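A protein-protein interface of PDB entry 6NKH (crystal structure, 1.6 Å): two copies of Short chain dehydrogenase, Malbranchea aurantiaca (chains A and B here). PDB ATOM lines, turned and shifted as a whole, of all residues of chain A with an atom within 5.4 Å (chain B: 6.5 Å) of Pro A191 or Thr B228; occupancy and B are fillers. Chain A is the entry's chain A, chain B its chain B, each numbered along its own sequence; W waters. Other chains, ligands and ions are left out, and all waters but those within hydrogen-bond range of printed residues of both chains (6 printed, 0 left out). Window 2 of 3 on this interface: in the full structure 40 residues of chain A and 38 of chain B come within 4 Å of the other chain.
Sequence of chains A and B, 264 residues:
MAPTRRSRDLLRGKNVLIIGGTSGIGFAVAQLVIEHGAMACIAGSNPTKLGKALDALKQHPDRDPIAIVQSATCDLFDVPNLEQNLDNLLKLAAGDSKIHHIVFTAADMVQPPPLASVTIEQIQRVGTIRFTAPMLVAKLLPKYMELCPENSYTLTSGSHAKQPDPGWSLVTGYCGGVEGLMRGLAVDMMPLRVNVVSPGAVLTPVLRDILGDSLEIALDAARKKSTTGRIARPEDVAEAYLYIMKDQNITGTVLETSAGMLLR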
ATOM      1  N   LEU A 147     -12.305  34.988  -8.074  1.00  0.00           N
ATOM      2  CA  LEU A 147     -11.328  34.423  -7.148  1.00  0.00           C
ATOM      3  C   LEU A 147     -11.972  33.222  -6.475  1.00  0.00           C
ATOM      4  O   LEU A 147     -12.597  33.332  -5.419  1.00  0.00           O
ATOM      5  CB  LEU A 147     -10.884  35.459  -6.127  1.00  0.00           C
ATOM      6  CG  LEU A 147     -10.224  36.710  -6.710  1.00  0.00           C
ATOM      7  CD1 LEU A 147      -9.813  37.649  -5.595  1.00  0.00           C
ATOM      8  CD2 LEU A 147      -9.044  36.355  -7.592  1.00  0.00           C
ATOM      9  N   CYS A 148     -11.833  32.062  -7.093  1.00  0.00           N
ATOM     10  CA  CYS A 148     -12.410  30.840  -6.562  1.00  0.00           C
ATOM     11  C   CYS A 148     -11.468  29.691  -6.876  1.00  0.00           C
ATOM     12  O   CYS A 148     -10.617  29.807  -7.760  1.00  0.00           O
ATOM     13  CB  CYS A 148     -13.807  30.592  -7.145  1.00  0.00           C
ATOM     14  SG  CYS A 148     -13.852  30.362  -8.920  1.00  0.00           S
ATOM     15  N   PRO A 149     -11.588  28.569  -6.150  1.00  0.00           N
ATOM     16  CA  PRO A 149     -10.661  27.446  -6.377  1.00  0.00           C
ATOM     17  C   PRO A 149     -10.927  26.652  -7.644  1.00  0.00           C
ATOM     18  O   PRO A 149     -10.111  25.786  -7.977  1.00  0.00           O
ATOM     19  CB  PRO A 149     -10.861  26.574  -5.133  1.00  0.00           C
ATOM     20  CG  PRO A 149     -12.227  26.886  -4.674  1.00  0.00           C
ATOM     21  CD  PRO A 149     -12.463  28.329  -4.991  1.00  0.00           C
ATOM     22  N   MET A 189      -4.655  36.362  -2.936  1.00  0.00           N
ATOM     23  CA  MET A 189      -5.738  36.201  -3.895  1.00  0.00           C
ATOM     24  C   MET A 189      -6.653  35.036  -3.553  1.00  0.00           C
ATOM     25  O   MET A 189      -7.465  34.630  -4.391  1.00  0.00           O
ATOM     26  CB  MET A 189      -5.176  36.020  -5.300  1.00  0.00           C
ATOM     27  CG  MET A 189      -4.301  37.171  -5.754  1.00  0.00           C
ATOM     28  SD  MET A 189      -3.832  36.967  -7.476  1.00  0.00           S
ATOM     29  CE  MET A 189      -5.371  37.436  -8.248  1.00  0.00           C
ATOM     30  N   MET A 190      -6.539  34.478  -2.356  1.00  0.00           N
ATOM     31  CA  MET A 190      -7.376  33.345  -2.009  1.00  0.00           C
ATOM     32  C   MET A 190      -8.845  33.759  -2.112  1.00  0.00           C
ATOM     33  O   MET A 190      -9.185  34.926  -1.878  1.00  0.00           O
ATOM     34  CB  MET A 190      -7.055  32.838  -0.604  1.00  0.00           C
ATOM     35  CG  MET A 190      -7.440  33.771   0.511  1.00  0.00           C
ATOM     36  SD  MET A 190      -7.090  33.085   2.141  1.00  0.00           S
ATOM     37  CE  MET A 190      -5.361  33.444   2.339  1.00  0.00           C
ATOM     38  N   PRO A 191      -9.747  32.822  -2.455  1.00  0.00           N
ATOM     39  CA  PRO A 191      -9.497  31.393  -2.661  1.00  0.00           C
ATOM     40  C   PRO A 191      -9.136  31.008  -4.096  1.00  0.00           C
ATOM     41  O   PRO A 191      -9.292  29.850  -4.463  1.00  0.00           O
ATOM     42  CB  PRO A 191     -10.825  30.760  -2.260  1.00  0.00           C
ATOM     43  CG  PRO A 191     -11.825  31.773  -2.677  1.00  0.00           C
ATOM     44  CD  PRO A 191     -11.186  33.125  -2.460  1.00  0.00           C
ATOM     45  N   LEU A 192      -8.677  31.960  -4.897  1.00  0.00           N
ATOM     46  CA  LEU A 192      -8.034  31.612  -6.155  1.00  0.00           C
ATOM     47  C   LEU A 192      -6.795  30.767  -5.879  1.00  0.00           C
ATOM     48  O   LEU A 192      -6.105  30.946  -4.871  1.00  0.00           O
ATOM     49  CB  LEU A 192      -7.635  32.865  -6.929  1.00  0.00           C
ATOM     50  CG  LEU A 192      -6.967  32.617  -8.284  1.00  0.00           C
ATOM     51  CD1 LEU A 192      -7.916  31.935  -9.248  1.00  0.00           C
ATOM     52  CD2 LEU A 192      -6.450  33.920  -8.856  1.00  0.00           C
ATOM     53  N   ARG A 193      -6.513  29.844  -6.794  1.00  0.00           N
ATOM     54  CA  ARG A 193      -5.363  28.951  -6.689  1.00  0.00           C
ATOM     55  C   ARG A 193      -4.227  29.502  -7.538  1.00  0.00           C
ATOM     56  O   ARG A 193      -4.432  29.838  -8.706  1.00  0.00           O
ATOM     57  CB  ARG A 193      -5.721  27.535  -7.140  1.00  0.00           C
ATOM     58  CG  ARG A 193      -6.776  26.863  -6.277  1.00  0.00           C
ATOM     59  CD  ARG A 193      -7.005  25.415  -6.667  1.00  0.00           C
ATOM     60  NE  ARG A 193      -7.545  25.271  -8.011  1.00  0.00           N
ATOM     61  CZ  ARG A 193      -6.873  24.771  -9.050  1.00  0.00           C
ATOM     62  NH1 ARG A 193      -5.614  24.367  -8.921  1.00  0.00           N
ATOM     63  NH2 ARG A 193      -7.465  24.681 -10.232  1.00  0.00           N
ATOM     64  N   GLN A 248      -8.628  21.101  -8.192  1.00  0.00           N
ATOM     65  CA  GLN A 248      -9.107  22.277  -7.484  1.00  0.00           C
ATOM     66  C   GLN A 248      -8.625  22.324  -6.045  1.00  0.00           C
ATOM     67  O   GLN A 248      -9.062  23.196  -5.284  1.00  0.00           O
ATOM     68  CB  GLN A 248     -10.632  22.316  -7.557  1.00  0.00           C
ATOM     69  CG  GLN A 248     -11.120  22.462  -8.991  1.00  0.00           C
ATOM     70  CD  GLN A 248     -12.630  22.403  -9.125  1.00  0.00           C
ATOM     71  OE1 GLN A 248     -13.348  22.193  -8.143  1.00  0.00           O
ATOM     72  NE2 GLN A 248     -13.117  22.578 -10.352  1.00  0.00           N
ATOM     73  N   ASN A 249      -7.717  21.421  -5.673  1.00  0.00           N
ATOM     74  CA  ASN A 249      -7.136  21.385  -4.342  1.00  0.00           C
ATOM     75  C   ASN A 249      -5.721  21.950  -4.288  1.00  0.00           C
ATOM     76  O   ASN A 249      -5.215  22.183  -3.192  1.00  0.00           O
ATOM     77  CB  ASN A 249      -7.059  19.948  -3.819  1.00  0.00           C
ATOM     78  CG  ASN A 249      -6.919  19.877  -2.315  1.00  0.00           C
ATOM     79  OD1 ASN A 249      -7.305  20.793  -1.602  1.00  0.00           O
ATOM     80  ND2 ASN A 249      -6.271  18.837  -1.837  1.00  0.00           N
ATOM     81  N   THR A 251      -2.716  24.482  -4.548  1.00  0.00           N
ATOM     82  CA  THR A 251      -2.348  25.887  -4.565  1.00  0.00           C
ATOM     83  C   THR A 251      -1.123  26.100  -3.689  1.00  0.00           C
ATOM     84  O   THR A 251      -0.901  25.375  -2.715  1.00  0.00           O
ATOM     85  CB  THR A 251      -3.500  26.793  -4.098  1.00  0.00           C
ATOM     86  OG1 THR A 251      -3.124  28.162  -4.267  1.00  0.00           O
ATOM     87  CG2 THR A 251      -3.864  26.540  -2.630  1.00  0.00           C
ATOM     88  N   ALA B 201      -6.272  17.815   3.283  1.00  0.00           N
ATOM     89  CA  ALA B 201      -7.633  18.361   3.264  1.00  0.00           C
ATOM     90  C   ALA B 201      -8.522  17.662   2.233  1.00  0.00           C
ATOM     91  O   ALA B 201      -9.249  18.305   1.475  1.00  0.00           O
ATOM     92  CB  ALA B 201      -7.615  19.873   3.007  1.00  0.00           C
ATOM     93  N   ARG B 223     -10.571  23.855   6.625  1.00  0.00           N
ATOM     94  CA  ARG B 223     -11.054  24.969   5.814  1.00  0.00           C
ATOM     95  C   ARG B 223     -10.419  26.285   6.236  1.00  0.00           C
ATOM     96  O   ARG B 223     -10.078  27.110   5.383  1.00  0.00           O
ATOM     97  CB  ARG B 223     -12.579  25.073   5.887  1.00  0.00           C
ATOM     98  CG  ARG B 223     -13.329  24.274   4.846  1.00  0.00           C
ATOM     99  CD  ARG B 223     -14.830  24.518   4.966  1.00  0.00           C
ATOM    100  NE  ARG B 223     -15.377  23.882   6.162  1.00  0.00           N
ATOM    101  CZ  ARG B 223     -16.084  22.751   6.174  1.00  0.00           C
ATOM    102  NH1 ARG B 223     -16.511  22.264   7.331  1.00  0.00           N
ATOM    103  NH2 ARG B 223     -16.415  22.133   5.045  1.00  0.00           N
ATOM    104  N   SER B 226      -6.662  26.262   5.203  1.00  0.00           N
ATOM    105  CA  SER B 226      -6.456  26.279   3.769  1.00  0.00           C
ATOM    106  C   SER B 226      -6.612  27.688   3.213  1.00  0.00           C
ATOM    107  O   SER B 226      -7.098  28.604   3.880  1.00  0.00           O
ATOM    108  CB  SER B 226      -7.459  25.361   3.089  1.00  0.00           C
ATOM    109  OG  SER B 226      -8.763  25.904   3.196  1.00  0.00           O
ATOM    110  N   THR B 227      -6.196  27.854   1.961  1.00  0.00           N
ATOM    111  CA  THR B 227      -6.504  29.055   1.207  1.00  0.00           C
ATOM    112  C   THR B 227      -7.637  28.853   0.212  1.00  0.00           C
ATOM    113  O   THR B 227      -8.207  29.842  -0.248  1.00  0.00           O
ATOM    114  CB  THR B 227      -5.267  29.549   0.458  1.00  0.00           C
ATOM    115  OG1 THR B 227      -4.802  28.512  -0.411  1.00  0.00           O
ATOM    116  CG2 THR B 227      -4.163  29.942   1.428  1.00  0.00           C
ATOM    117  N   THR B 228      -7.966  27.603  -0.143  1.00  0.00           N
ATOM    118  CA  THR B 228      -9.160  27.345  -0.950  1.00  0.00           C
ATOM    119  C   THR B 228     -10.443  27.482  -0.136  1.00  0.00           C
ATOM    120  O   THR B 228     -11.523  27.580  -0.724  1.00  0.00           O
ATOM    121  CB  THR B 228      -9.124  25.943  -1.567  1.00  0.00           C
ATOM    122  OG1 THR B 228      -9.126  24.951  -0.534  1.00  0.00           O
ATOM    123  CG2 THR B 228      -7.902  25.774  -2.457  1.00  0.00           C
ATOM    124  N   GLY B 229     -10.338  27.490   1.190  1.00  0.00           N
ATOM    125  CA  GLY B 229     -11.506  27.558   2.044  1.00  0.00           C
ATOM    126  C   GLY B 229     -12.460  26.412   1.833  1.00  0.00           C
ATOM    127  O   GLY B 229     -13.665  26.558   2.070  1.00  0.00           O
ATOM    128  N   ARG B 230     -11.953  25.260   1.403  1.00  0.00           N
ATOM    129  CA  ARG B 230     -12.829  24.203   0.928  1.00  0.00           C
ATOM    130  C   ARG B 230     -12.166  22.853   1.132  1.00  0.00           C
ATOM    131  O   ARG B 230     -10.987  22.683   0.817  1.00  0.00           O
ATOM    132  CB  ARG B 230     -13.155  24.431  -0.546  1.00  0.00           C
ATOM    133  CG  ARG B 230     -14.303  23.631  -1.033  1.00  0.00           C
ATOM    134  CD  ARG B 230     -14.657  24.011  -2.443  1.00  0.00           C
ATOM    135  NE  ARG B 230     -13.720  23.489  -3.427  1.00  0.00           N
ATOM    136  CZ  ARG B 230     -13.741  23.825  -4.711  1.00  0.00           C
ATOM    137  NH1 ARG B 230     -14.639  24.697  -5.155  1.00  0.00           N
ATOM    138  NH2 ARG B 230     -12.870  23.293  -5.554  1.00  0.00           N
ATOM    139  N   ILE B 231     -12.917  21.900   1.678  1.00  0.00           N
ATOM    140  CA  ILE B 231     -12.424  20.535   1.750  1.00  0.00           C
ATOM    141  C   ILE B 231     -12.424  19.947   0.351  1.00  0.00           C
ATOM    142  O   ILE B 231     -13.334  20.202  -0.452  1.00  0.00           O
ATOM    143  CB  ILE B 231     -13.270  19.681   2.701  1.00  0.00           C
ATOM    144  CG1 ILE B 231     -13.252  20.271   4.110  1.00  0.00           C
ATOM    145  CG2 ILE B 231     -12.735  18.271   2.735  1.00  0.00           C
ATOM    146  CD1 ILE B 231     -11.879  20.313   4.752  1.00  0.00           C
ATOM    147  N   ALA B 232     -11.404  19.153   0.054  1.00  0.00           N
ATOM    148  CA  ALA B 232     -11.210  18.616  -1.280  1.00  0.00           C
ATOM    149  C   ALA B 232     -11.822  17.227  -1.404  1.00  0.00           C
ATOM    150  O   ALA B 232     -11.897  16.469  -0.432  1.00  0.00           O
ATOM    151  CB  ALA B 232      -9.721  18.564  -1.611  1.00  0.00           C
ATOM    152  N   SER B 258      -2.674  20.165  -1.243  1.00  0.00           N
ATOM    153  CA  SER B 258      -3.144  20.238   0.139  1.00  0.00           C
ATOM    154  C   SER B 258      -3.815  21.573   0.466  1.00  0.00           C
ATOM    155  O   SER B 258      -3.751  22.036   1.607  1.00  0.00           O
ATOM    156  CB  SER B 258      -1.987  19.962   1.098  1.00  0.00           C
ATOM    157  OG  SER B 258      -0.884  20.803   0.834  1.00  0.00           O
ATOM    158  N   ALA B 259      -4.438  22.204  -0.531  1.00  0.00           N
ATOM    159  CA  ALA B 259      -5.394  23.304  -0.386  1.00  0.00           C
ATOM    160  C   ALA B 259      -4.788  24.600   0.113  1.00  0.00           C
ATOM    161  O   ALA B 259      -5.532  25.520   0.481  1.00  0.00           O
ATOM    162  CB  ALA B 259      -6.542  22.933   0.553  1.00  0.00           C
ATOM    163  N   GLY B 260      -3.465  24.712   0.135  1.00  0.00           N
ATOM    164  CA  GLY B 260      -2.807  25.893   0.624  1.00  0.00           C
ATOM    165  C   GLY B 260      -2.518  25.885   2.106  1.00  0.00           C
ATOM    166  O   GLY B 260      -2.015  26.882   2.624  1.00  0.00           O
ATOM    167  N   ARG B 264       0.262  28.392   5.576  1.00  0.00           N
ATOM    168  CA  ARG B 264      -0.243  29.040   6.779  1.00  0.00           C
ATOM    169  C   ARG B 264       0.214  28.249   7.997  1.00  0.00           C
ATOM    170  O   ARG B 264       0.502  27.057   7.920  1.00  0.00           O
ATOM    171  CB  ARG B 264      -1.775  29.169   6.681  1.00  0.00           C
ATOM    172  CG  ARG B 264      -2.159  29.805   5.349  1.00  0.00           C
ATOM    173  CD  ARG B 264      -3.617  29.958   5.044  1.00  0.00           C
ATOM    174  NE  ARG B 264      -4.236  31.108   5.675  1.00  0.00           N
ATOM    175  CZ  ARG B 264      -5.524  31.394   5.545  1.00  0.00           C
ATOM    176  NH1 ARG B 264      -6.302  30.636   4.784  1.00  0.00           N
ATOM    177  NH2 ARG B 264      -6.034  32.449   6.150  1.00  0.00           N
ATOM    178  OXT ARG B 264       0.356  28.815   9.076  1.00  0.00           O
HETATM  179  O   HOH W   1      -1.321  22.364  -2.551  1.00  0.00           O
HETATM  180  O   HOH W   2     -10.192  30.906   2.033  1.00  0.00           O
HETATM  181  O   HOH W   3     -11.073  22.873  -3.601  1.00  0.00           O
HETATM  182  O   HOH W   4      -4.679  30.129  -2.928  1.00  0.00           O
HETATM  183  O   HOH W   5      -9.423  22.367  -1.192  1.00  0.00           O
HETATM  184  O   HOH W   6     -13.372  20.673  -5.039  1.00  0.00           O
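Water W4 lies within hydrogen-bond range of O of Leu A192 (2.5 Å), OG1 of Thr A251 (2.8 Å) and OG1 of Thr B227 (3.0 Å). Water W5 lies within hydrogen-bond range of O of Arg B230 (2.6 Å), OD1 of Asn A249 (2.7 Å) and OG1 of Thr B228 (2.7 Å). Water W3 lies within hydrogen-bond range of O of Gln A248 (2.6 Å) and NH2 of Arg B230 (2.7 Å). Water W6 lies within hydrogen-bond range of NH2 of Arg B230 (2.7 Å) and OE1 of Gln A248 (3.5 Å). Water W1 bridges the backbone NH (N) of Ser B258 (2.9 Å) and the backbone carbonyl oxygen (O) of Thr A251 (3.0 Å). Water W2 bridges O of Thr B227 (3.2 Å) and SD of Met A190 (3.8 Å).
Printed residues of chain A that touch a printed residue of chain B: Pro A149, Met A190, Pro A191, Gln A248, Asn A249 and Thr A251. Hydrophobic or aromatic side chains of chain A that line the printed part of chain B: Pro A149, Met A190 and Pro A191. Hydrophobic or aromatic side chains of chain B that line the printed part of chain A: Ala B232 and Ala B259. Among the printed residues, no Asp or Glu carboxylate lies within 4 Å of a Lys or Arg side-chain nitrogen of the other chain.
Printed residues of chain B within 4 Å of Pro A149: Arg B230 (3.3 Å). Printed residues of chain B within 4 Å of Met A190: Thr B227 and Arg B264. Printed residues of chain B within 4 Å of Pro A191: Thr B227 (3.1 Å) and Thr B228 (3.6 Å). Of the printed residues of chain B, Gln A248 touches Thr B228 and Arg B230. Of the printed residues of chain A, Thr B228 touches Pro A191 and Gln A248. Printed residues of chain A within 4 Å of Ala B259: Asn A249 and Thr A251. The nearest residue of chain B that does not touch Pro A191 is Gly B229 (4.8 Å). The nearest printed residue of chain B that does not touch Pro A149 is Thr B228 (4.02 Å).
Among the printed residues, merely in contact across the chains: Pro A149 with Arg B230 (3.3 Å), Met A190 with Thr B227 (3.2 Å), Pro A191 with Thr B227 (3.1 Å), Pro A191 with Thr B228 (3.6 Å), Gln A248 with Thr B228 (3.998 Å), Asn A249 with Ala B232 (3.2 Å), Asn A249 with Ser B258 (3.8 Å), Thr A251 with Thr B227 (3.1 Å), Thr A251 with Ala B259 (3.5 Å) and Thr A251 with Gly B260 (3.3 Å).
O of Pro A149 sits at hydrogen-bond distance from NE of Arg A193. The backbone carbonyl oxygen (O) of Ala B201 lies within hydrogen-bond range of the backbone NH (N) of Ala B232, 2.7 Å away. The backbone carbonyl oxygen (O) of Ala B259 is in hydrogen-bond range of the backbone NH (N) of Thr B227 (2.8 Å). The side-chain hydroxyl of Thr B228 lies within hydrogen-bond range of the backbone carbonyl oxygen of Arg B230 (3.2 Å). The backbone NH (N) of Thr B228 lies within hydrogen-bond range of the backbone carbonyl oxygen (O) of Ala B259 (3.3 Å).
No position is printed for both chains.
The guanidinium group (NH1) of Arg B264 lies within hydrogen-bond range of the side-chain sulfur (SD) of Met A190 (3.7 Å). The side-chain amide oxygen (OE1) of Gln A248 lies within hydrogen-bond range of the guanidinium group (NH2) of Arg B230, 2.9 Å away. The backbone carbonyl oxygen (O) of Asn A249 lies within hydrogen-bond range of the backbone NH (N) of Ala B259 (2.8 Å).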
